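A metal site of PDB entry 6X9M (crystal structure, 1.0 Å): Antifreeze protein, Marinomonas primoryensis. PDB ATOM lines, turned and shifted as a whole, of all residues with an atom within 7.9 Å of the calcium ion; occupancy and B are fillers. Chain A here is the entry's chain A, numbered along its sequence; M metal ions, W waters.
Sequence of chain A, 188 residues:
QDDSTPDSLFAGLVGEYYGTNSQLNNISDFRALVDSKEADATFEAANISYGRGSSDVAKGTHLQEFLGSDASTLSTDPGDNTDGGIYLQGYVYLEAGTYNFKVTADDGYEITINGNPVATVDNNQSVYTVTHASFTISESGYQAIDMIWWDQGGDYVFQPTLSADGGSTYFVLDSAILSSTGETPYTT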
ATOM      1  N   THR A  20     -12.337 -25.476  -2.385  1.00  0.00           N
ATOM      2  CA  THR A  20     -11.406 -25.655  -3.501  1.00  0.00           C
ATOM      3  C   THR A  20     -10.636 -24.363  -3.720  1.00  0.00           C
ATOM      4  O   THR A  20     -11.104 -23.272  -3.394  1.00  0.00           O
ATOM      5  CB  THR A  20     -12.159 -26.082  -4.781  1.00  0.00           C
ATOM      6  OG1 THR A  20     -11.236 -26.353  -5.852  1.00  0.00           O
ATOM      7  CG2 THR A  20     -13.141 -25.038  -5.285  1.00  0.00           C
ATOM      8  N   ASN A  21      -9.470 -24.496  -4.358  1.00  0.00           N
ATOM      9  CA  ASN A  21      -8.710 -23.326  -4.823  1.00  0.00           C
ATOM     10  C   ASN A  21      -8.803 -23.135  -6.324  1.00  0.00           C
ATOM     11  O   ASN A  21      -8.085 -22.295  -6.900  1.00  0.00           O
ATOM     12  CB  ASN A  21      -7.264 -23.418  -4.330  1.00  0.00           C
ATOM     13  CG  ASN A  21      -7.204 -23.513  -2.837  1.00  0.00           C
ATOM     14  OD1 ASN A  21      -7.935 -22.807  -2.121  1.00  0.00           O
ATOM     15  ND2 ASN A  21      -6.350 -24.405  -2.326  1.00  0.00           N
ATOM     16  N   SER A  22      -9.693 -23.858  -6.971  1.00  0.00           N
ATOM     17  CA  SER A  22     -10.129 -23.598  -8.340  1.00  0.00           C
ATOM     18  C   SER A  22     -11.366 -22.706  -8.355  1.00  0.00           C
ATOM     19  O   SER A  22     -12.041 -22.528  -7.330  1.00  0.00           O
ATOM     20  CB  SER A  22     -10.424 -24.927  -9.052  1.00  0.00           C
ATOM     21  OG  SER A  22     -11.587 -25.562  -8.547  1.00  0.00           O
ATOM     22  N   GLN A  23     -11.659 -22.142  -9.535  1.00  0.00           N
ATOM     23  CA  GLN A  23     -12.807 -21.256  -9.664  1.00  0.00           C
ATOM     24  C   GLN A  23     -14.091 -22.060  -9.859  1.00  0.00           C
ATOM     25  O   GLN A  23     -14.169 -22.940 -10.724  1.00  0.00           O
ATOM     26  CB  GLN A  23     -12.599 -20.331 -10.859  1.00  0.00           C
ATOM     27  CG  GLN A  23     -13.829 -19.548 -11.300  1.00  0.00           C
ATOM     28  CD  GLN A  23     -14.305 -18.490 -10.316  1.00  0.00           C
ATOM     29  OE1 GLN A  23     -13.865 -18.424  -9.176  1.00  0.00           O
ATOM     30  NE2 GLN A  23     -15.252 -17.663 -10.753  1.00  0.00           N
ATOM     31  N   LEU A  24     -15.107 -21.701  -9.091  1.00  0.00           N
ATOM     32  CA  LEU A  24     -16.458 -22.212  -9.285  1.00  0.00           C
ATOM     33  C   LEU A  24     -17.257 -21.190 -10.093  1.00  0.00           C
ATOM     34  O   LEU A  24     -17.529 -20.089  -9.619  1.00  0.00           O
ATOM     35  CB  LEU A  24     -17.110 -22.466  -7.938  1.00  0.00           C
ATOM     36  CG  LEU A  24     -16.436 -23.548  -7.083  1.00  0.00           C
ATOM     37  CD1 LEU A  24     -17.090 -23.611  -5.722  1.00  0.00           C
ATOM     38  CD2 LEU A  24     -16.447 -24.894  -7.752  1.00  0.00           C
ATOM     39  N   ASN A  25     -17.616 -21.557 -11.328  1.00  0.00           N
ATOM     40  CA  ASN A  25     -18.375 -20.660 -12.203  1.00  0.00           C
ATOM     41  C   ASN A  25     -19.838 -21.026 -12.350  1.00  0.00           C
ATOM     42  O   ASN A  25     -20.628 -20.186 -12.791  1.00  0.00           O
ATOM     43  CB  ASN A  25     -17.781 -20.627 -13.616  1.00  0.00           C
ATOM     44  CG  ASN A  25     -16.550 -19.759 -13.706  1.00  0.00           C
ATOM     45  OD1 ASN A  25     -16.527 -18.634 -13.203  1.00  0.00           O
ATOM     46  ND2 ASN A  25     -15.500 -20.285 -14.327  1.00  0.00           N
ATOM     47  N   ASP A  56     -15.123 -14.125   1.607  1.00  0.00           N
ATOM     48  CA  ASP A  56     -15.003 -15.502   1.097  1.00  0.00           C
ATOM     49  C   ASP A  56     -15.536 -16.547   2.098  1.00  0.00           C
ATOM     50  O   ASP A  56     -15.024 -16.662   3.215  1.00  0.00           O
ATOM     51  CB  ASP A  56     -13.572 -15.909   0.763  1.00  0.00           C
ATOM     52  CG  ASP A  56     -12.848 -14.946  -0.144  1.00  0.00           C
ATOM     53  OD1 ASP A  56     -13.461 -14.320  -1.027  1.00  0.00           O
ATOM     54  OD2 ASP A  56     -11.616 -14.878  -0.005  1.00  0.00           O
ATOM     55  N   THR A  82     -10.146 -20.821  -1.504  1.00  0.00           N
ATOM     56  CA  THR A  82     -10.647 -19.592  -2.112  1.00  0.00           C
ATOM     57  C   THR A  82     -12.146 -19.650  -2.398  1.00  0.00           C
ATOM     58  O   THR A  82     -12.837 -18.623  -2.313  1.00  0.00           O
ATOM     59  CB  THR A  82      -9.899 -19.282  -3.421  1.00  0.00           C
ATOM     60  OG1 THR A  82     -10.153 -20.271  -4.421  1.00  0.00           O
ATOM     61  CG2 THR A  82      -8.392 -19.223  -3.199  1.00  0.00           C
ATOM     62  N   ASP A  83     -12.665 -20.832  -2.738  1.00  0.00           N
ATOM     63  CA  ASP A  83     -14.032 -21.041  -3.206  1.00  0.00           C
ATOM     64  C   ASP A  83     -14.614 -22.204  -2.413  1.00  0.00           C
ATOM     65  O   ASP A  83     -13.876 -23.083  -1.945  1.00  0.00           O
ATOM     66  CB  ASP A  83     -14.031 -21.433  -4.717  1.00  0.00           C
ATOM     67  CG  ASP A  83     -13.587 -20.300  -5.654  1.00  0.00           C
ATOM     68  OD1 ASP A  83     -12.528 -19.683  -5.422  1.00  0.00           O
ATOM     69  OD2 ASP A  83     -14.303 -20.054  -6.668  1.00  0.00           O
ATOM     70  N   GLY A  84     -15.935 -22.246  -2.260  1.00  0.00           N
ATOM     71  CA  GLY A  84     -16.514 -23.388  -1.553  1.00  0.00           C
ATOM     72  C   GLY A  84     -18.016 -23.376  -1.668  1.00  0.00           C
ATOM     73  O   GLY A  84     -18.627 -22.407  -2.104  1.00  0.00           O
ATOM     74  N   ASP A 107     -23.307 -17.112  -4.280  1.00  0.00           N
ATOM     75  CA  ASP A 107     -23.435 -17.048  -5.740  1.00  0.00           C
ATOM     76  C   ASP A 107     -24.660 -17.853  -6.173  1.00  0.00           C
ATOM     77  O   ASP A 107     -25.767 -17.487  -5.802  1.00  0.00           O
ATOM     78  CB  ASP A 107     -22.093 -17.468  -6.349  1.00  0.00           C
ATOM     79  CG  ASP A 107     -21.080 -16.362  -6.225  1.00  0.00           C
ATOM     80  OD1 ASP A 107     -21.171 -15.413  -7.061  1.00  0.00           O
ATOM     81  OD2 ASP A 107     -20.209 -16.391  -5.300  1.00  0.00           O
ATOM     82  N   ASN A 124     -22.453 -17.201 -11.289  1.00  0.00           N
ATOM     83  CA  ASN A 124     -22.107 -16.350 -10.157  1.00  0.00           C
ATOM     84  C   ASN A 124     -22.936 -15.082 -10.186  1.00  0.00           C
ATOM     85  O   ASN A 124     -23.421 -14.668 -11.246  1.00  0.00           O
ATOM     86  CB  ASN A 124     -20.620 -16.051 -10.203  1.00  0.00           C
ATOM     87  CG  ASN A 124     -19.805 -17.272  -9.856  1.00  0.00           C
ATOM     88  OD1 ASN A 124     -20.224 -18.076  -9.005  1.00  0.00           O
ATOM     89  ND2 ASN A 124     -18.639 -17.436 -10.485  1.00  0.00           N
ATOM     90  N   TRP A 150     -23.023 -22.381  -3.894  1.00  0.00           N
ATOM     91  CA  TRP A 150     -21.598 -22.122  -3.750  1.00  0.00           C
ATOM     92  C   TRP A 150     -21.299 -20.619  -3.709  1.00  0.00           C
ATOM     93  O   TRP A 150     -22.136 -19.786  -4.073  1.00  0.00           O
ATOM     94  CB  TRP A 150     -20.764 -22.821  -4.871  1.00  0.00           C
ATOM     95  CG  TRP A 150     -20.866 -22.075  -6.181  1.00  0.00           C
ATOM     96  CD1 TRP A 150     -20.040 -21.088  -6.629  1.00  0.00           C
ATOM     97  CD2 TRP A 150     -21.895 -22.201  -7.170  1.00  0.00           C
ATOM     98  NE1 TRP A 150     -20.503 -20.600  -7.828  1.00  0.00           N
ATOM     99  CE2 TRP A 150     -21.650 -21.252  -8.169  1.00  0.00           C
ATOM    100  CE3 TRP A 150     -23.010 -23.030  -7.288  1.00  0.00           C
ATOM    101  CZ2 TRP A 150     -22.470 -21.112  -9.284  1.00  0.00           C
ATOM    102  CZ3 TRP A 150     -23.832 -22.871  -8.380  1.00  0.00           C
ATOM    103  CH2 TRP A 150     -23.561 -21.917  -9.367  1.00  0.00           C
ATOM    104  N   ASP A 151     -20.061 -20.338  -3.298  1.00  0.00           N
ATOM    105  CA  ASP A 151     -19.445 -19.019  -3.299  1.00  0.00           C
ATOM    106  C   ASP A 151     -18.142 -19.101  -4.101  1.00  0.00           C
ATOM    107  O   ASP A 151     -17.248 -19.895  -3.774  1.00  0.00           O
ATOM    108  CB  ASP A 151     -19.117 -18.567  -1.862  1.00  0.00           C
ATOM    109  CG  ASP A 151     -18.377 -17.249  -1.817  1.00  0.00           C
ATOM    110  OD1 ASP A 151     -18.700 -16.387  -2.657  1.00  0.00           O
ATOM    111  OD2 ASP A 151     -17.454 -17.099  -0.965  1.00  0.00           O
ATOM    112  N   GLN A 152     -18.036 -18.284  -5.142  1.00  0.00           N
ATOM    113  CA  GLN A 152     -16.792 -18.152  -5.889  1.00  0.00           C
ATOM    114  C   GLN A 152     -15.804 -17.212  -5.213  1.00  0.00           C
ATOM    115  O   GLN A 152     -14.660 -17.096  -5.676  1.00  0.00           O
ATOM    116  CB  GLN A 152     -17.085 -17.648  -7.306  1.00  0.00           C
ATOM    117  CG  GLN A 152     -17.558 -16.203  -7.387  1.00  0.00           C
ATOM    118  CD  GLN A 152     -16.453 -15.223  -7.716  1.00  0.00           C
ATOM    119  OE1 GLN A 152     -15.712 -15.411  -8.689  1.00  0.00           O
ATOM    120  NE2 GLN A 152     -16.365 -14.159  -6.932  1.00  0.00           N
ATOM    121  N   GLY A 153     -16.228 -16.541  -4.145  1.00  0.00           N
ATOM    122  CA  GLY A 153     -15.431 -15.539  -3.466  1.00  0.00           C
ATOM    123  C   GLY A 153     -16.268 -14.292  -3.190  1.00  0.00           C
ATOM    124  O   GLY A 153     -17.310 -14.077  -3.817  1.00  0.00           O
ATOM    125  N   GLY A 154     -15.786 -13.471  -2.262  1.00  0.00           N
ATOM    126  CA  GLY A 154     -16.460 -12.220  -1.932  1.00  0.00           C
ATOM    127  C   GLY A 154     -17.560 -12.431  -0.902  1.00  0.00           C
ATOM    128  O   GLY A 154     -17.331 -13.035   0.145  1.00  0.00           O
HETATM  129 CA    CA M   1     -12.997 -17.951  -7.075  1.00  0.00          CA
HETATM  130  O   HOH W   1     -11.040 -18.619  -8.211  1.00  0.00           O
HETATM  131  O   HOH W   2     -11.482 -16.617  -5.803  1.00  0.00           O
HETATM  132  O   HOH W   3     -13.301 -15.719  -8.015  1.00  0.00           O
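The calcium ion is bound by OE1 of Gln 23, O of Gln 152, water W1, water W2, OD1 of Asp 83, water W3 and OD2 of Asp 83.
The calcium ion has seven donor atoms within binding distance.
Within 4 Å of the calcium ion: Gln 23, Asp 83 and Gln 152.
The nearest printed residue that does not touch the calcium ion is Thr 82 (4.5 Å).
The side-chain amide nitrogen of Gln 23 lies close to the side-chain amide nitrogen of Asn 124, at 3.4 Å.
The side-chain amide nitrogen of Gln 23 is in hydrogen-bond range of the side-chain amide oxygen of Asn 25, at 2.9 Å.
N of Gln 152 lies close to OD2 of Asp 107 (2.9 Å).
OD1 of Asp 83 lies close to OG1 of Thr 82 (2.6 Å).
The side-chain carboxylate (OD2) of Asp 83 sits close to the backbone NH (N) of Leu 24 (3.0 Å).
O of Asp 83 sits at hydrogen-bond distance from N of Thr 20 (2.9 Å).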
